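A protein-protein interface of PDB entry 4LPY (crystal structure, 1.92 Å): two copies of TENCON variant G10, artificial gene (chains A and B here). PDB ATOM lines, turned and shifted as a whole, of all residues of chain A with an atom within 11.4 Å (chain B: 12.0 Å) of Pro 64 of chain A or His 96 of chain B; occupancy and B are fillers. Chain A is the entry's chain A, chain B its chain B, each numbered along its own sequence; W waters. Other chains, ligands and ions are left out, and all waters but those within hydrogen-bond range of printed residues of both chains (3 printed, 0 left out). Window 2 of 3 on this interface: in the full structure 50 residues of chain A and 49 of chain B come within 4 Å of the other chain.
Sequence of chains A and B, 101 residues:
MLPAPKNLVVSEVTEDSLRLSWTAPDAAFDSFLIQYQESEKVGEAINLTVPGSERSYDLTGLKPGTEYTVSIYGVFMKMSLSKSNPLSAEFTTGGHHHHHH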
ATOM      1  N   VAL A  13     -10.586  16.624  33.575  1.00  0.00           N
ATOM      2  CA  VAL A  13      -9.279  17.153  33.187  1.00  0.00           C
ATOM      3  C   VAL A  13      -8.928  18.265  34.171  1.00  0.00           C
ATOM      4  O   VAL A  13      -9.796  19.061  34.565  1.00  0.00           O
ATOM      5  CB  VAL A  13      -9.318  17.759  31.764  1.00  0.00           C
ATOM      6  CG1 VAL A  13      -8.033  18.515  31.444  1.00  0.00           C
ATOM      7  CG2 VAL A  13      -9.594  16.678  30.709  1.00  0.00           C
ATOM      8  N   THR A  14      -7.662  18.318  34.566  1.00  0.00           N
ATOM      9  CA  THR A  14      -7.138  19.474  35.278  1.00  0.00           C
ATOM     10  C   THR A  14      -5.859  19.950  34.578  1.00  0.00           C
ATOM     11  O   THR A  14      -5.459  19.413  33.533  1.00  0.00           O
ATOM     12  CB  THR A  14      -6.869  19.197  36.780  1.00  0.00           C
ATOM     13  OG1 THR A  14      -5.698  18.378  36.922  1.00  0.00           O
ATOM     14  CG2 THR A  14      -8.068  18.512  37.450  1.00  0.00           C
ATOM     15  N   GLU A  15      -5.213  20.958  35.152  1.00  0.00           N
ATOM     16  CA  GLU A  15      -3.965  21.455  34.579  1.00  0.00           C
ATOM     17  C   GLU A  15      -2.808  20.460  34.660  1.00  0.00           C
ATOM     18  O   GLU A  15      -1.784  20.672  34.013  1.00  0.00           O
ATOM     19  CB  GLU A  15      -3.570  22.780  35.216  1.00  0.00           C
ATOM     20  CG  GLU A  15      -4.546  23.877  34.890  1.00  0.00           C
ATOM     21  CD  GLU A  15      -4.510  24.989  35.903  1.00  0.00           C
ATOM     22  OE1 GLU A  15      -3.528  25.759  35.887  1.00  0.00           O
ATOM     23  OE2 GLU A  15      -5.462  25.089  36.710  1.00  0.00           O
ATOM     24  N   ASP A  16      -2.965  19.389  35.441  1.00  0.00           N
ATOM     25  CA  ASP A  16      -1.907  18.380  35.537  1.00  0.00           C
ATOM     26  C   ASP A  16      -2.428  16.948  35.580  1.00  0.00           C
ATOM     27  O   ASP A  16      -1.722  16.038  36.016  1.00  0.00           O
ATOM     28  CB  ASP A  16      -0.997  18.657  36.736  1.00  0.00           C
ATOM     29  CG  ASP A  16      -1.747  18.632  38.056  1.00  0.00           C
ATOM     30  OD1 ASP A  16      -2.708  17.846  38.183  1.00  0.00           O
ATOM     31  OD2 ASP A  16      -1.376  19.396  38.965  1.00  0.00           O
ATOM     32  N   SER A  17      -3.661  16.737  35.130  1.00  0.00           N
ATOM     33  CA  SER A  17      -4.228  15.380  35.155  1.00  0.00           C
ATOM     34  C   SER A  17      -5.301  15.141  34.093  1.00  0.00           C
ATOM     35  O   SER A  17      -5.963  16.081  33.610  1.00  0.00           O
ATOM     36  CB  SER A  17      -4.754  15.027  36.559  1.00  0.00           C
ATOM     37  OG  SER A  17      -5.881  15.829  36.924  1.00  0.00           O
ATOM     38  N   LEU A  18      -5.454  13.866  33.745  1.00  0.00           N
ATOM     39  CA  LEU A  18      -6.506  13.383  32.860  1.00  0.00           C
ATOM     40  C   LEU A  18      -7.096  12.155  33.533  1.00  0.00           C
ATOM     41  O   LEU A  18      -6.402  11.145  33.709  1.00  0.00           O
ATOM     42  CB  LEU A  18      -5.938  12.998  31.495  1.00  0.00           C
ATOM     43  CG  LEU A  18      -5.236  14.072  30.672  1.00  0.00           C
ATOM     44  CD1 LEU A  18      -4.534  13.457  29.454  1.00  0.00           C
ATOM     45  CD2 LEU A  18      -6.264  15.109  30.258  1.00  0.00           C
ATOM     46  N   GLU A  38       3.348  12.678  25.735  1.00  0.00           N
ATOM     47  CA  GLU A  38       3.032  13.914  25.034  1.00  0.00           C
ATOM     48  C   GLU A  38       2.974  13.626  23.530  1.00  0.00           C
ATOM     49  O   GLU A  38       3.835  12.925  22.992  1.00  0.00           O
ATOM     50  CB  GLU A  38       4.049  15.017  25.377  1.00  0.00           C
ATOM     51  CG  GLU A  38       4.051  15.387  26.847  1.00  0.00           C
ATOM     52  CD  GLU A  38       5.247  16.227  27.246  1.00  0.00           C
ATOM     53  OE1 GLU A  38       5.504  17.245  26.577  1.00  0.00           O
ATOM     54  OE2 GLU A  38       5.932  15.868  28.230  1.00  0.00           O
ATOM     55  N   SER A  39       1.959  14.164  22.862  1.00  0.00           N
ATOM     56  CA  SER A  39       1.708  13.839  21.453  1.00  0.00           C
ATOM     57  C   SER A  39       2.867  14.194  20.506  1.00  0.00           C
ATOM     58  O   SER A  39       3.119  13.472  19.549  1.00  0.00           O
ATOM     59  CB  SER A  39       0.414  14.508  20.961  1.00  0.00           C
ATOM     60  OG  SER A  39      -0.701  13.985  21.658  1.00  0.00           O
ATOM     61  N   VAL A  42       7.546  14.971  23.112  1.00  0.00           N
ATOM     62  CA  VAL A  42       8.360  15.578  24.168  1.00  0.00           C
ATOM     63  C   VAL A  42       8.165  14.727  25.419  1.00  0.00           C
ATOM     64  O   VAL A  42       7.055  14.262  25.674  1.00  0.00           O
ATOM     65  CB  VAL A  42       7.929  17.038  24.477  1.00  0.00           C
ATOM     66  CG1 VAL A  42       9.018  17.781  25.254  1.00  0.00           C
ATOM     67  CG2 VAL A  42       7.560  17.796  23.202  1.00  0.00           C
ATOM     68  N   LEU A  59      -4.547   9.739  35.208  1.00  0.00           N
ATOM     69  CA  LEU A  59      -3.175  10.071  34.803  1.00  0.00           C
ATOM     70  C   LEU A  59      -2.821  11.376  35.462  1.00  0.00           C
ATOM     71  O   LEU A  59      -3.517  12.373  35.275  1.00  0.00           O
ATOM     72  CB  LEU A  59      -3.043  10.220  33.286  1.00  0.00           C
ATOM     73  CG  LEU A  59      -3.409   9.046  32.382  1.00  0.00           C
ATOM     74  CD1 LEU A  59      -3.155   9.469  30.960  1.00  0.00           C
ATOM     75  CD2 LEU A  59      -2.604   7.784  32.726  1.00  0.00           C
ATOM     76  N   THR A  60      -1.738  11.377  36.237  1.00  0.00           N
ATOM     77  CA  THR A  60      -1.398  12.537  37.063  1.00  0.00           C
ATOM     78  C   THR A  60       0.027  13.014  36.786  1.00  0.00           C
ATOM     79  O   THR A  60       0.809  12.322  36.115  1.00  0.00           O
ATOM     80  CB  THR A  60      -1.563  12.220  38.571  1.00  0.00           C
ATOM     81  OG1 THR A  60      -0.710  11.127  38.925  1.00  0.00           O
ATOM     82  CG2 THR A  60      -3.023  11.869  38.912  1.00  0.00           C
ATOM     83  N   GLY A  61       0.349  14.196  37.309  1.00  0.00           N
ATOM     84  CA  GLY A  61       1.685  14.776  37.210  1.00  0.00           C
ATOM     85  C   GLY A  61       2.034  15.238  35.816  1.00  0.00           C
ATOM     86  O   GLY A  61       3.194  15.203  35.433  1.00  0.00           O
ATOM     87  N   LEU A  62       1.021  15.668  35.064  1.00  0.00           N
ATOM     88  CA  LEU A  62       1.189  16.079  33.680  1.00  0.00           C
ATOM     89  C   LEU A  62       1.527  17.563  33.591  1.00  0.00           C
ATOM     90  O   LEU A  62       1.474  18.283  34.584  1.00  0.00           O
ATOM     91  CB  LEU A  62      -0.085  15.763  32.870  1.00  0.00           C
ATOM     92  CG  LEU A  62      -0.602  14.319  32.974  1.00  0.00           C
ATOM     93  CD1 LEU A  62      -1.866  14.135  32.145  1.00  0.00           C
ATOM     94  CD2 LEU A  62       0.492  13.286  32.562  1.00  0.00           C
ATOM     95  N   LYS A  63       1.875  17.997  32.390  1.00  0.00           N
ATOM     96  CA  LYS A  63       2.167  19.383  32.094  1.00  0.00           C
ATOM     97  C   LYS A  63       0.881  20.069  31.641  1.00  0.00           C
ATOM     98  O   LYS A  63       0.070  19.445  30.955  1.00  0.00           O
ATOM     99  CB  LYS A  63       3.181  19.450  30.961  1.00  0.00           C
ATOM    100  CG  LYS A  63       4.574  18.939  31.357  1.00  0.00           C
ATOM    101  CD  LYS A  63       5.422  18.709  30.121  1.00  0.00           C
ATOM    102  CE  LYS A  63       6.832  18.288  30.487  1.00  0.00           C
ATOM    103  NZ  LYS A  63       7.664  18.141  29.265  1.00  0.00           N
ATOM    104  N   PRO A  64       0.694  21.343  32.023  1.00  0.00           N
ATOM    105  CA  PRO A  64      -0.479  22.110  31.582  1.00  0.00           C
ATOM    106  C   PRO A  64      -0.512  22.431  30.089  1.00  0.00           C
ATOM    107  O   PRO A  64       0.536  22.492  29.438  1.00  0.00           O
ATOM    108  CB  PRO A  64      -0.391  23.395  32.422  1.00  0.00           C
ATOM    109  CG  PRO A  64       1.077  23.551  32.715  1.00  0.00           C
ATOM    110  CD  PRO A  64       1.577  22.137  32.907  1.00  0.00           C
ATOM    111  N   GLY A  65      -1.721  22.631  29.566  1.00  0.00           N
ATOM    112  CA  GLY A  65      -1.960  22.954  28.161  1.00  0.00           C
ATOM    113  C   GLY A  65      -1.272  22.060  27.146  1.00  0.00           C
ATOM    114  O   GLY A  65      -0.797  22.531  26.103  1.00  0.00           O
ATOM    115  N   THR A  66      -1.214  20.767  27.447  1.00  0.00           N
ATOM    116  CA  THR A  66      -0.391  19.851  26.678  1.00  0.00           C
ATOM    117  C   THR A  66      -1.222  18.676  26.165  1.00  0.00           C
ATOM    118  O   THR A  66      -1.994  18.066  26.914  1.00  0.00           O
ATOM    119  CB  THR A  66       0.815  19.367  27.533  1.00  0.00           C
ATOM    120  OG1 THR A  66       1.622  20.496  27.885  1.00  0.00           O
ATOM    121  CG2 THR A  66       1.668  18.333  26.773  1.00  0.00           C
ATOM    122  N   GLU A  67      -1.049  18.377  24.881  1.00  0.00           N
ATOM    123  CA  GLU A  67      -1.706  17.254  24.243  1.00  0.00           C
ATOM    124  C   GLU A  67      -0.936  15.951  24.513  1.00  0.00           C
ATOM    125  O   GLU A  67       0.303  15.886  24.356  1.00  0.00           O
ATOM    126  CB  GLU A  67      -1.866  17.505  22.740  1.00  0.00           C
ATOM    127  CG  GLU A  67      -2.877  16.585  22.084  1.00  0.00           C
ATOM    128  CD  GLU A  67      -2.904  16.724  20.572  1.00  0.00           C
ATOM    129  OE1 GLU A  67      -3.210  17.829  20.075  1.00  0.00           O
ATOM    130  OE2 GLU A  67      -2.617  15.724  19.881  1.00  0.00           O
ATOM    131  N   TYR A  68      -1.694  14.932  24.919  1.00  0.00           N
ATOM    132  CA  TYR A  68      -1.185  13.581  25.209  1.00  0.00           C
ATOM    133  C   TYR A  68      -1.892  12.554  24.331  1.00  0.00           C
ATOM    134  O   TYR A  68      -3.102  12.643  24.106  1.00  0.00           O
ATOM    135  CB  TYR A  68      -1.427  13.235  26.688  1.00  0.00           C
ATOM    136  CG  TYR A  68      -0.485  13.976  27.612  1.00  0.00           C
ATOM    137  CD1 TYR A  68      -0.825  15.236  28.115  1.00  0.00           C
ATOM    138  CD2 TYR A  68       0.741  13.421  27.981  1.00  0.00           C
ATOM    139  CE1 TYR A  68       0.035  15.924  28.965  1.00  0.00           C
ATOM    140  CE2 TYR A  68       1.615  14.105  28.836  1.00  0.00           C
ATOM    141  CZ  TYR A  68       1.244  15.356  29.316  1.00  0.00           C
ATOM    142  OH  TYR A  68       2.076  16.052  30.155  1.00  0.00           O
ATOM    143  N   PHE B  91      -5.795  13.669  24.205  1.00  0.00           N
ATOM    144  CA  PHE B  91      -6.471  14.553  25.168  1.00  0.00           C
ATOM    145  C   PHE B  91      -5.559  15.714  25.545  1.00  0.00           C
ATOM    146  O   PHE B  91      -4.343  15.550  25.600  1.00  0.00           O
ATOM    147  CB  PHE B  91      -6.856  13.796  26.456  1.00  0.00           C
ATOM    148  CG  PHE B  91      -7.752  12.605  26.226  1.00  0.00           C
ATOM    149  CD1 PHE B  91      -9.102  12.777  25.908  1.00  0.00           C
ATOM    150  CD2 PHE B  91      -7.246  11.300  26.328  1.00  0.00           C
ATOM    151  CE1 PHE B  91      -9.934  11.676  25.695  1.00  0.00           C
ATOM    152  CE2 PHE B  91      -8.067  10.192  26.118  1.00  0.00           C
ATOM    153  CZ  PHE B  91      -9.411  10.375  25.801  1.00  0.00           C
ATOM    154  N   THR B  92      -6.141  16.882  25.803  1.00  0.00           N
ATOM    155  CA  THR B  92      -5.352  18.038  26.244  1.00  0.00           C
ATOM    156  C   THR B  92      -5.615  18.384  27.698  1.00  0.00           C
ATOM    157  O   THR B  92      -6.766  18.488  28.129  1.00  0.00           O
ATOM    158  CB  THR B  92      -5.640  19.259  25.359  1.00  0.00           C
ATOM    159  OG1 THR B  92      -5.478  18.885  23.987  1.00  0.00           O
ATOM    160  CG2 THR B  92      -4.712  20.396  25.683  1.00  0.00           C
ATOM    161  N   THR B  93      -4.534  18.564  28.455  1.00  0.00           N
ATOM    162  CA  THR B  93      -4.642  18.955  29.833  1.00  0.00           C
ATOM    163  C   THR B  93      -5.117  20.411  29.889  1.00  0.00           C
ATOM    164  O   THR B  93      -5.037  21.144  28.891  1.00  0.00           O
ATOM    165  CB  THR B  93      -3.292  18.814  30.589  1.00  0.00           C
ATOM    166  OG1 THR B  93      -2.268  19.491  29.855  1.00  0.00           O
ATOM    167  CG2 THR B  93      -2.919  17.321  30.751  1.00  0.00           C
ATOM    168  N   GLY B  94      -5.605  20.798  31.060  1.00  0.00           N
ATOM    169  CA  GLY B  94      -6.110  22.153  31.292  1.00  0.00           C
ATOM    170  C   GLY B  94      -4.990  23.172  31.346  1.00  0.00           C
ATOM    171  O   GLY B  94      -3.809  22.819  31.485  1.00  0.00           O
ATOM    172  N   GLY B  95      -5.360  24.443  31.234  1.00  0.00           N
ATOM    173  CA  GLY B  95      -4.419  25.523  31.469  1.00  0.00           C
ATOM    174  C   GLY B  95      -3.625  25.958  30.251  1.00  0.00           C
ATOM    175  O   GLY B  95      -3.864  25.509  29.123  1.00  0.00           O
ATOM    176  N   HIS B  96      -2.668  26.846  30.494  1.00  0.00           N
ATOM    177  CA  HIS B  96      -1.879  27.432  29.422  1.00  0.00           C
ATOM    178  C   HIS B  96      -0.568  26.688  29.240  1.00  0.00           C
ATOM    179  O   HIS B  96       0.099  26.346  30.215  1.00  0.00           O
ATOM    180  CB  HIS B  96      -1.651  28.928  29.687  1.00  0.00           C
ATOM    181  CG  HIS B  96      -2.920  29.727  29.721  1.00  0.00           C
ATOM    182  ND1 HIS B  96      -3.470  30.201  30.892  1.00  0.00           N
ATOM    183  CD2 HIS B  96      -3.748  30.133  28.725  1.00  0.00           C
ATOM    184  CE1 HIS B  96      -4.580  30.865  30.618  1.00  0.00           C
ATOM    185  NE2 HIS B  96      -4.770  30.838  29.310  1.00  0.00           N
ATOM    186  N   HIS B  97      -0.216  26.444  27.983  1.00  0.00           N
ATOM    187  CA  HIS B  97       1.046  25.805  27.634  1.00  0.00           C
ATOM    188  C   HIS B  97       2.190  26.766  27.954  1.00  0.00           C
ATOM    189  O   HIS B  97       2.067  27.973  27.731  1.00  0.00           O
ATOM    190  CB  HIS B  97       1.051  25.423  26.150  1.00  0.00           C
ATOM    191  CG  HIS B  97       2.319  24.761  25.704  1.00  0.00           C
ATOM    192  ND1 HIS B  97       2.566  23.417  25.896  1.00  0.00           N
ATOM    193  CD2 HIS B  97       3.411  25.259  25.077  1.00  0.00           C
ATOM    194  CE1 HIS B  97       3.755  23.117  25.405  1.00  0.00           C
ATOM    195  NE2 HIS B  97       4.288  24.216  24.902  1.00  0.00           N
ATOM    196  N   HIS B  98       3.293  26.232  28.473  1.00  0.00           N
ATOM    197  CA  HIS B  98       4.467  27.046  28.795  1.00  0.00           C
ATOM    198  C   HIS B  98       5.753  26.438  28.229  1.00  0.00           C
ATOM    199  O   HIS B  98       5.982  25.230  28.325  1.00  0.00           O
ATOM    200  CB  HIS B  98       4.583  27.245  30.305  1.00  0.00           C
HETATM  201  O   HOH W   1       3.165  23.382  29.493  1.00  0.00           O
HETATM  202  O   HOH W   2       4.238  20.806  27.385  1.00  0.00           O
HETATM  203  O   HOH W   3      -2.230  27.193  33.207  1.00  0.00           O
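The backbone carbonyl oxygen (O) of Gly 94 of chain B lies within hydrogen-bond range of the backbone NH (N) of Gly 65 of chain A (2.8 Å). N of Thr 66 of chain A sits at hydrogen-bond distance from OG1 of Thr 93 of chain B (2.9 Å). N of Gly 65 of chain A sits at hydrogen-bond distance from OG1 of Thr 93 of chain B. The backbone NH (N) of Tyr 68 of chain A is in hydrogen-bond range of the backbone carbonyl oxygen (O) of Phe 91 of chain B (2.8 Å). O of Thr 14 of chain A is in hydrogen-bond range of N of Gly 94 of chain B, 2.8 Å away. The backbone carbonyl oxygen (O) of Lys 63 of chain A is in hydrogen-bond range of the side-chain hydroxyl (OG1) of Thr 93 of chain B (2.6 Å). The backbone carbonyl oxygen of Gly 65 of chain A sits close to a ring nitrogen (ND1) of His 97 of chain B, at 3.5 Å.
O of Asp 16 of chain A is in hydrogen-bond range of N of Leu 62 of chain A, at 2.9 Å. N of Lys 63 of chain A lies within hydrogen-bond range of OH of Tyr 68 of chain A (3.0 Å). The backbone carbonyl oxygen (O) of Glu 67 of chain A is in hydrogen-bond range of the backbone NH (N) of Ser 39 of chain A (2.8 Å). N of Asp 16 of chain A sits close to OG1 of Thr 14 of chain A (3.3 Å). The backbone carbonyl oxygen (O) of Leu 18 of chain A is in hydrogen-bond range of the backbone NH (N) of Leu 59 of chain A (2.8 Å). OG1 of Thr 14 of chain A is in hydrogen-bond range of OG of Ser 17 of chain A.
Among the printed residues, pairs that only touch across the chains: Gly 65 of chain A with Gly 95 of chain B, Val 13 of chain A with Gly 94 of chain B, Glu 15 of chain A with Gly 94 of chain B, Pro 64 of chain A with Gly 94 of chain B, Glu 67 of chain A with Phe 91 of chain B, Thr 66 of chain A with Thr 92 of chain B, Pro 64 of chain A with Thr 93 of chain B, Val 13 of chain A with Thr 92 of chain B, Leu 62 of chain A with Thr 93 of chain B, Thr 66 of chain A with His 97 of chain B, Thr 66 of chain A with Phe 91 of chain B, Thr 14 of chain A with Thr 93 of chain B, Pro 64 of chain A with His 96 of chain B, Tyr 68 of chain A with Thr 93 of chain B, Val 13 of chain A with Thr 93 of chain B, Glu 15 of chain A with Gly 95 of chain B, Pro 64 of chain A with His 97 of chain B, Leu 18 of chain A with Phe 91 of chain B, Glu 67 of chain A with Thr 92 of chain B and Leu 18 of chain A with Thr 93 of chain B.
Of chain B, only Thr 93, Gly 94, His 96 and His 97 come within 4 Å of Pro 64 of chain A. Of chain A, only Pro 64 comes within 4 Å of His 96 of chain B. Of chain B, only Thr 93 (3.2 Å), Gly 94 (2.8 Å), Gly 95 (3.3 Å) and His 97 (3.4 Å) come within 4 Å of Gly 65 of chain A. Thr 66 of chain A touches just these residues of chain B: Phe 91, Thr 92, Thr 93 and His 97. Gly 94 of chain B touches just these residues of chain A: Val 13 (3.4 Å), Thr 14 (2.8 Å), Glu 15 (3.4 Å), Pro 64 (3.4 Å) and Gly 65 (2.8 Å). His 97 of chain B touches just these residues of chain A: Pro 64, Gly 65 and Thr 66. No residue of chain A comes within 4 Å of His 98 of chain B. Of the printed residues of chain B, Glu 67 of chain A touches Phe 91 and Thr 92. Of the printed residues of chain A, Thr 92 of chain B touches Val 13 (3.5 Å), Thr 66 (3.4 Å) and Glu 67 (3.96 Å). The nearest residue of chain A that does not touch His 96 of chain B is Gly 65 of chain A (4.1 Å).
Of the 8 printed residues of chain B, 7 touch a printed residue of chain A. Printed residues of chain A that touch a printed residue of chain B: Val 13, Thr 14, Glu 15, Leu 18, Leu 62, Lys 63, Pro 64, Gly 65, Thr 66, Glu 67 and Tyr 68. Along chain A the printed residues that touch a printed residue of chain B span positions 13 to 68. Among the printed residues, 27 pairs touch across the chains.
No position is printed for both chains. Of the 27 pairs that touch across the chains among the printed residues, none has its exchanged pair printed and touching as well.
Water W2 bridges OG1 of Thr 66 of chain A (2.7 Å) and ND1 of His 97 of chain B (3.4 Å). Water W3 lies within hydrogen-bond range of N of His 96 of chain B (2.8 Å) and OE1 of Glu 15 of chain A (3.3 Å). Water W1 bridges O of Pro 64 of chain A and N of His 98 of chain B.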
